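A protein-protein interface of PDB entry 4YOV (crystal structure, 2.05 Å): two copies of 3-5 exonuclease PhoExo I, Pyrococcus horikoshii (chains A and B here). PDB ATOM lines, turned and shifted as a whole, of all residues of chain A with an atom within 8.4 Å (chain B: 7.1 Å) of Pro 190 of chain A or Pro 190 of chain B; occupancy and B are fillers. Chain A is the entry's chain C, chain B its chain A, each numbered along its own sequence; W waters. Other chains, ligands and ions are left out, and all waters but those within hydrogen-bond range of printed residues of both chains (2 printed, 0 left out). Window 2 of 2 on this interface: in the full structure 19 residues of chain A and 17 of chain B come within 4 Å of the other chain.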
ATOM      1  N   ARG A 142     -24.318  20.155  16.487  1.00  0.00           N
ATOM      2  CA  ARG A 142     -24.031  18.716  16.451  1.00  0.00           C
ATOM      3  C   ARG A 142     -23.164  18.305  17.655  1.00  0.00           C
ATOM      4  O   ARG A 142     -23.338  17.225  18.229  1.00  0.00           O
ATOM      5  CB  ARG A 142     -23.344  18.312  15.137  1.00  0.00           C
ATOM      6  CG  ARG A 142     -22.801  16.813  15.140  1.00  0.00           C
ATOM      7  CD  ARG A 142     -23.908  15.777  15.325  1.00  0.00           C
ATOM      8  NE  ARG A 142     -23.410  14.397  15.085  1.00  0.00           N
ATOM      9  CZ  ARG A 142     -24.054  13.295  15.458  1.00  0.00           C
ATOM     10  NH1 ARG A 142     -25.200  13.401  16.118  1.00  0.00           N
ATOM     11  NH2 ARG A 142     -23.537  12.075  15.197  1.00  0.00           N
ATOM     12  N   TYR A 173     -26.368   8.449  15.057  1.00  0.00           N
ATOM     13  CA  TYR A 173     -25.044   7.936  14.722  1.00  0.00           C
ATOM     14  C   TYR A 173     -23.889   8.523  15.520  1.00  0.00           C
ATOM     15  O   TYR A 173     -22.953   9.108  14.986  1.00  0.00           O
ATOM     16  CB  TYR A 173     -24.763   8.060  13.198  1.00  0.00           C
ATOM     17  CG  TYR A 173     -25.131   9.354  12.473  1.00  0.00           C
ATOM     18  CD1 TYR A 173     -24.264  10.444  12.468  1.00  0.00           C
ATOM     19  CD2 TYR A 173     -26.310   9.454  11.744  1.00  0.00           C
ATOM     20  CE1 TYR A 173     -24.591  11.653  11.787  1.00  0.00           C
ATOM     21  CE2 TYR A 173     -26.646  10.645  11.046  1.00  0.00           C
ATOM     22  CZ  TYR A 173     -25.779  11.726  11.072  1.00  0.00           C
ATOM     23  OH  TYR A 173     -26.104  12.884  10.390  1.00  0.00           O
ATOM     24  N   SER A 187     -18.819  11.172  17.077  1.00  0.00           N
ATOM     25  CA  SER A 187     -19.698  10.975  15.935  1.00  0.00           C
ATOM     26  C   SER A 187     -19.248   9.739  15.207  1.00  0.00           C
ATOM     27  O   SER A 187     -18.049   9.535  15.045  1.00  0.00           O
ATOM     28  CB  SER A 187     -19.677  12.157  14.980  1.00  0.00           C
ATOM     29  OG  SER A 187     -20.545  11.920  13.880  1.00  0.00           O
ATOM     30  N   LEU A 188     -20.192   8.955  14.702  1.00  0.00           N
ATOM     31  CA  LEU A 188     -19.812   7.805  13.880  1.00  0.00           C
ATOM     32  C   LEU A 188     -19.638   8.193  12.416  1.00  0.00           C
ATOM     33  O   LEU A 188     -19.203   7.372  11.594  1.00  0.00           O
ATOM     34  CB  LEU A 188     -20.854   6.685  13.991  1.00  0.00           C
ATOM     35  CG  LEU A 188     -20.857   5.920  15.308  1.00  0.00           C
ATOM     36  CD1 LEU A 188     -22.104   5.072  15.359  1.00  0.00           C
ATOM     37  CD2 LEU A 188     -19.608   5.033  15.441  1.00  0.00           C
ATOM     38  N   ASP A 189     -19.973   9.437  12.081  1.00  0.00           N
ATOM     39  CA  ASP A 189     -19.888   9.880  10.679  1.00  0.00           C
ATOM     40  C   ASP A 189     -18.558  10.552  10.407  1.00  0.00           C
ATOM     41  O   ASP A 189     -18.331  11.668  10.841  1.00  0.00           O
ATOM     42  CB  ASP A 189     -21.020  10.847  10.337  1.00  0.00           C
ATOM     43  CG  ASP A 189     -21.116  11.147   8.821  1.00  0.00           C
ATOM     44  OD1 ASP A 189     -20.234  10.703   8.047  1.00  0.00           O
ATOM     45  OD2 ASP A 189     -22.076  11.837   8.404  1.00  0.00           O
ATOM     46  N   PRO A 190     -17.658   9.872   9.699  1.00  0.00           N
ATOM     47  CA  PRO A 190     -16.390  10.555   9.439  1.00  0.00           C
ATOM     48  C   PRO A 190     -16.521  11.768   8.499  1.00  0.00           C
ATOM     49  O   PRO A 190     -15.587  12.576   8.434  1.00  0.00           O
ATOM     50  CB  PRO A 190     -15.537   9.478   8.780  1.00  0.00           C
ATOM     51  CG  PRO A 190     -16.555   8.498   8.156  1.00  0.00           C
ATOM     52  CD  PRO A 190     -17.747   8.537   9.072  1.00  0.00           C
ATOM     53  N   ARG A 191     -17.632  11.894   7.767  1.00  0.00           N
ATOM     54  CA  ARG A 191     -17.828  13.091   6.946  1.00  0.00           C
ATOM     55  C   ARG A 191     -17.853  14.386   7.783  1.00  0.00           C
ATOM     56  O   ARG A 191     -17.573  15.458   7.269  1.00  0.00           O
ATOM     57  CB  ARG A 191     -19.123  12.985   6.170  1.00  0.00           C
ATOM     58  CG  ARG A 191     -19.136  11.830   5.128  1.00  0.00           C
ATOM     59  CD  ARG A 191     -20.471  11.734   4.468  1.00  0.00           C
ATOM     60  NE  ARG A 191     -21.592  11.609   5.399  1.00  0.00           N
ATOM     61  CZ  ARG A 191     -22.850  11.854   5.036  1.00  0.00           C
ATOM     62  NH1 ARG A 191     -23.105  12.237   3.790  1.00  0.00           N
ATOM     63  NH2 ARG A 191     -23.850  11.728   5.895  1.00  0.00           N
ATOM     64  N   GLU A 192     -18.149  14.267   9.076  1.00  0.00           N
ATOM     65  CA  GLU A 192     -18.282  15.439   9.961  1.00  0.00           C
ATOM     66  C   GLU A 192     -16.932  15.942  10.443  1.00  0.00           C
ATOM     67  O   GLU A 192     -16.828  17.034  11.043  1.00  0.00           O
ATOM     68  CB  GLU A 192     -19.182  15.111  11.161  1.00  0.00           C
ATOM     69  CG  GLU A 192     -20.643  14.892  10.772  1.00  0.00           C
ATOM     70  CD  GLU A 192     -21.578  14.744  11.965  1.00  0.00           C
ATOM     71  OE1 GLU A 192     -22.792  15.032  11.800  1.00  0.00           O
ATOM     72  OE2 GLU A 192     -21.119  14.336  13.059  1.00  0.00           O
ATOM     73  N   GLY A 193     -15.897  15.148  10.195  1.00  0.00           N
ATOM     74  CA  GLY A 193     -14.542  15.605  10.398  1.00  0.00           C
ATOM     75  C   GLY A 193     -13.996  15.395  11.809  1.00  0.00           C
ATOM     76  O   GLY A 193     -13.068  16.093  12.195  1.00  0.00           O
ATOM     77  N   GLY A 194     -14.586  14.475  12.576  1.00  0.00           N
ATOM     78  CA  GLY A 194     -14.024  14.046  13.849  1.00  0.00           C
ATOM     79  C   GLY A 194     -14.556  14.789  15.068  1.00  0.00           C
ATOM     80  O   GLY A 194     -13.778  15.248  15.883  1.00  0.00           O
ATOM     81  N   LEU A 195     -15.878  14.896  15.177  1.00  0.00           N
ATOM     82  CA  LEU A 195     -16.540  15.612  16.263  1.00  0.00           C
ATOM     83  C   LEU A 195     -16.636  14.719  17.493  1.00  0.00           C
ATOM     84  O   LEU A 195     -17.035  13.559  17.377  1.00  0.00           O
ATOM     85  CB  LEU A 195     -17.932  16.064  15.837  1.00  0.00           C
ATOM     86  CG  LEU A 195     -17.961  16.825  14.513  1.00  0.00           C
ATOM     87  CD1 LEU A 195     -19.385  17.187  14.120  1.00  0.00           C
ATOM     88  CD2 LEU A 195     -17.077  18.054  14.605  1.00  0.00           C
ATOM     89  N   TYR B 173     -17.298  17.059   2.303  1.00  0.00           N
ATOM     90  CA  TYR B 173     -16.650  15.982   3.046  1.00  0.00           C
ATOM     91  C   TYR B 173     -15.469  15.374   2.340  1.00  0.00           C
ATOM     92  O   TYR B 173     -15.514  14.241   1.872  1.00  0.00           O
ATOM     93  CB  TYR B 173     -17.667  14.917   3.457  1.00  0.00           C
ATOM     94  CG  TYR B 173     -18.713  14.481   2.464  1.00  0.00           C
ATOM     95  CD1 TYR B 173     -18.429  13.521   1.502  1.00  0.00           C
ATOM     96  CD2 TYR B 173     -20.018  14.950   2.553  1.00  0.00           C
ATOM     97  CE1 TYR B 173     -19.389  13.090   0.610  1.00  0.00           C
ATOM     98  CE2 TYR B 173     -20.991  14.520   1.667  1.00  0.00           C
ATOM     99  CZ  TYR B 173     -20.657  13.587   0.697  1.00  0.00           C
ATOM    100  OH  TYR B 173     -21.600  13.135  -0.180  1.00  0.00           O
ATOM    101  N   SER B 187     -11.879  11.485  -0.393  1.00  0.00           N
ATOM    102  CA  SER B 187     -13.224  11.647   0.155  1.00  0.00           C
ATOM    103  C   SER B 187     -13.216  11.248   1.626  1.00  0.00           C
ATOM    104  O   SER B 187     -12.455  10.375   2.004  1.00  0.00           O
ATOM    105  CB  SER B 187     -14.247  10.795  -0.585  1.00  0.00           C
ATOM    106  OG  SER B 187     -15.537  10.969  -0.020  1.00  0.00           O
ATOM    107  N   LEU B 188     -14.008  11.919   2.460  1.00  0.00           N
ATOM    108  CA  LEU B 188     -14.192  11.455   3.837  1.00  0.00           C
ATOM    109  C   LEU B 188     -15.321  10.427   3.953  1.00  0.00           C
ATOM    110  O   LEU B 188     -15.564   9.922   5.036  1.00  0.00           O
ATOM    111  CB  LEU B 188     -14.457  12.644   4.792  1.00  0.00           C
ATOM    112  CG  LEU B 188     -13.211  13.425   5.161  1.00  0.00           C
ATOM    113  CD1 LEU B 188     -13.577  14.736   5.845  1.00  0.00           C
ATOM    114  CD2 LEU B 188     -12.356  12.556   6.107  1.00  0.00           C
ATOM    115  N   ASP B 189     -16.049  10.160   2.863  1.00  0.00           N
ATOM    116  CA  ASP B 189     -17.175   9.224   2.920  1.00  0.00           C
ATOM    117  C   ASP B 189     -16.761   7.820   2.441  1.00  0.00           C
ATOM    118  O   ASP B 189     -16.590   7.611   1.248  1.00  0.00           O
ATOM    119  CB  ASP B 189     -18.355   9.726   2.083  1.00  0.00           C
ATOM    120  CG  ASP B 189     -19.627   8.895   2.280  1.00  0.00           C
ATOM    121  OD1 ASP B 189     -19.566   7.830   2.938  1.00  0.00           O
ATOM    122  OD2 ASP B 189     -20.700   9.320   1.786  1.00  0.00           O
ATOM    123  N   PRO B 190     -16.629   6.860   3.374  1.00  0.00           N
ATOM    124  CA  PRO B 190     -16.235   5.486   2.984  1.00  0.00           C
ATOM    125  C   PRO B 190     -17.287   4.763   2.114  1.00  0.00           C
ATOM    126  O   PRO B 190     -16.955   3.784   1.439  1.00  0.00           O
ATOM    127  CB  PRO B 190     -16.033   4.775   4.335  1.00  0.00           C
ATOM    128  CG  PRO B 190     -16.814   5.585   5.346  1.00  0.00           C
ATOM    129  CD  PRO B 190     -16.764   7.026   4.837  1.00  0.00           C
ATOM    130  N   ARG B 191     -18.524   5.256   2.108  1.00  0.00           N
ATOM    131  CA  ARG B 191     -19.540   4.716   1.219  1.00  0.00           C
ATOM    132  C   ARG B 191     -19.194   4.917  -0.263  1.00  0.00           C
ATOM    133  O   ARG B 191     -19.753   4.232  -1.121  1.00  0.00           O
ATOM    134  CB  ARG B 191     -20.904   5.327   1.525  1.00  0.00           C
ATOM    135  CG  ARG B 191     -21.401   5.004   2.926  1.00  0.00           C
ATOM    136  CD  ARG B 191     -22.723   5.711   3.187  1.00  0.00           C
ATOM    137  NE  ARG B 191     -22.609   7.145   2.898  1.00  0.00           N
ATOM    138  CZ  ARG B 191     -23.648   7.957   2.718  1.00  0.00           C
ATOM    139  NH1 ARG B 191     -24.887   7.492   2.789  1.00  0.00           N
ATOM    140  NH2 ARG B 191     -23.448   9.234   2.454  1.00  0.00           N
ATOM    141  N   GLU B 192     -18.297   5.851  -0.569  1.00  0.00           N
ATOM    142  CA  GLU B 192     -17.960   6.135  -1.966  1.00  0.00           C
ATOM    143  C   GLU B 192     -16.908   5.173  -2.508  1.00  0.00           C
ATOM    144  O   GLU B 192     -16.654   5.143  -3.710  1.00  0.00           O
ATOM    145  CB  GLU B 192     -17.496   7.581  -2.135  1.00  0.00           C
ATOM    146  CG  GLU B 192     -18.632   8.550  -1.888  1.00  0.00           C
ATOM    147  CD  GLU B 192     -18.286  10.013  -2.133  1.00  0.00           C
ATOM    148  OE1 GLU B 192     -19.247  10.782  -2.363  1.00  0.00           O
ATOM    149  OE2 GLU B 192     -17.096  10.409  -2.036  1.00  0.00           O
ATOM    150  N   GLY B 193     -16.289   4.404  -1.616  1.00  0.00           N
ATOM    151  CA  GLY B 193     -15.461   3.276  -2.034  1.00  0.00           C
ATOM    152  C   GLY B 193     -14.015   3.652  -2.267  1.00  0.00           C
ATOM    153  O   GLY B 193     -13.284   2.953  -2.969  1.00  0.00           O
ATOM    154  N   GLY B 194     -13.599   4.782  -1.693  1.00  0.00           N
ATOM    155  CA  GLY B 194     -12.185   5.125  -1.637  1.00  0.00           C
ATOM    156  C   GLY B 194     -11.694   6.023  -2.758  1.00  0.00           C
ATOM    157  O   GLY B 194     -10.663   5.755  -3.389  1.00  0.00           O
ATOM    158  N   ARG B 219     -20.201  18.935   7.569  1.00  0.00           N
ATOM    159  CA  ARG B 219     -19.634  18.017   6.569  1.00  0.00           C
ATOM    160  C   ARG B 219     -18.796  18.717   5.505  1.00  0.00           C
ATOM    161  O   ARG B 219     -18.412  18.084   4.528  1.00  0.00           O
ATOM    162  CB  ARG B 219     -20.733  17.160   5.907  1.00  0.00           C
ATOM    163  CG  ARG B 219     -21.367  16.215   6.906  1.00  0.00           C
ATOM    164  CD  ARG B 219     -22.295  15.205   6.266  1.00  0.00           C
ATOM    165  NE  ARG B 219     -23.474  15.867   5.728  1.00  0.00           N
ATOM    166  CZ  ARG B 219     -24.579  16.104   6.428  1.00  0.00           C
ATOM    167  NH1 ARG B 219     -24.657  15.749   7.708  1.00  0.00           N
ATOM    168  NH2 ARG B 219     -25.604  16.714   5.846  1.00  0.00           N
ATOM    169  N   MET B 221     -15.079  20.852   5.123  1.00  0.00           N
ATOM    170  CA  MET B 221     -13.867  21.204   5.872  1.00  0.00           C
ATOM    171  C   MET B 221     -13.280  22.532   5.389  1.00  0.00           C
ATOM    172  O   MET B 221     -13.547  22.985   4.262  1.00  0.00           O
ATOM    173  CB  MET B 221     -12.818  20.089   5.744  1.00  0.00           C
ATOM    174  CG  MET B 221     -13.294  18.725   6.223  1.00  0.00           C
ATOM    175  SD  MET B 221     -13.651  18.690   7.996  1.00  0.00           S
ATOM    176  CE  MET B 221     -15.436  18.478   7.981  1.00  0.00           C
HETATM  177  O   HOH W   1     -18.777  18.747  10.196  1.00  0.00           O
HETATM  178  O   HOH W   2     -23.693  13.843   9.253  1.00  0.00           O
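Pro 190 of chain A touches its own counterpart, Pro 190 of chain B.
Arg 191 of chain A touches Tyr 173 of chain B, but with the chains exchanged Tyr 173 of chain A does not touch Arg 191 of chain B (9.0 Å).
Arg 191 of chain A touches Leu 188 of chain B, but with the chains exchanged Leu 188 of chain A does not touch Arg 191 of chain B (9.3 Å).
Arg 191 of chain A touches its own counterpart, Arg 191 of chain B.
Positions printed for both chains: 173, 187, 188, 189, 190, 191, 192, 193 and 194.
Of the 11 pairs that touch across the chains among the printed residues, 2 have their exchanged pair printed and touching as well.
Hydrophobic or aromatic side chains of chain A within 4 Å of the printed part of chain B: Pro 190.
Printed residues of chain B that touch a printed residue of chain A: Tyr 173, Leu 188, Asp 189, Pro 190, Arg 191, Arg 219 and Met 221.
Hydrophobic or aromatic side chains of chain B that line the printed part of chain A: Tyr 173, Leu 188, Pro 190 and Met 221.
Among the printed residues, 11 pairs touch across the chains.
Among the printed residues, no Asp or Glu carboxylate lies within 4 Å of a Lys or Arg side-chain nitrogen of the other chain.
The backbone NH of Leu 188 of chain B sits at hydrogen-bond distance from the backbone carbonyl oxygen of Tyr 173 of chain B (2.8 Å).
The backbone NH (N) of Tyr 173 of chain B sits at hydrogen-bond distance from the backbone carbonyl oxygen (O) of Arg 219 of chain B (2.7 Å).
The side-chain hydroxyl of Ser 187 of chain B sits at hydrogen-bond distance from the backbone NH of Asp 189 of chain B, 3.0 Å away.
The side-chain carboxylate (OD2) of Asp 189 of chain B is in salt-bridge range of the guanidinium group (NH2) of Arg 191 of chain B (2.8 Å).
The side-chain hydroxyl (OG) of Ser 187 of chain A sits at hydrogen-bond distance from the backbone NH (N) of Asp 189 of chain A (3.1 Å).
The side-chain hydroxyl (OG) of Ser 187 of chain A lies within hydrogen-bond range of the side-chain carboxylate (OE2) of Glu 192 of chain A (2.6 Å).
Gly 194 of chain A touches none of the printed residues of chain B.
Printed residues of chain A within 4 Å of Tyr 173 of chain B: Arg 191 (3.6 Å).
Of the printed residues of chain A, Asp 189 of chain B touches Arg 191.
Of chain A, only Pro 190 comes within 4 Å of Pro 190 of chain B.
Of the printed residues of chain A, Arg 191 of chain B touches Arg 191.
The nearest printed residue of chain A that does not touch Met 221 of chain B is Pro 190 of chain A (5.9 Å).
Arg 219 of chain B touches Asp 189 of chain A.
O of Leu 188 of chain B touches CG of Pro 190 of chain A, at 3.6 Å.
CG of Pro 190 of chain A touches CD of Pro 190 of chain B (3.6 Å).
CB of Arg 191 of chain A touches CB of Tyr 173 of chain B (3.6 Å).
O of Leu 188 of chain B touches N of Arg 191 of chain A (3.95 Å).
Arg 191 of chain A touches Asp 189 of chain B.
CA of Arg 219 of chain B touches O of Arg 191 of chain A, at 3.4 Å.
Met 221 of chain B touches Arg 191 of chain A (CE to O, 3.8 Å).
Met 221 of chain B touches Glu 192 of chain A (CE to O, 3.7 Å).
CA of Gly 193 of chain A touches CE of Met 221 of chain B, 3.9 Å away.
Water W2 lies within hydrogen-bond range of the guanidinium group (NH1) of Arg 219 of chain B (2.6 Å), the side-chain carboxylate (OD2) of Asp 189 of chain A (2.7 Å), the side-chain hydroxyl (OH) of Tyr 173 of chain A (2.8 Å) and the side-chain carboxylate (OE1) of Glu 192 of chain A (3.0 Å).
Water W1 bridges O of Glu 192 of chain A (2.7 Å) and N of Arg 219 of chain B (3.0 Å).
The guanidinium group (NH2) of Arg 191 of chain B sits close to the guanidinium group (NH1) of Arg 191 of chain A (3.3 Å).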
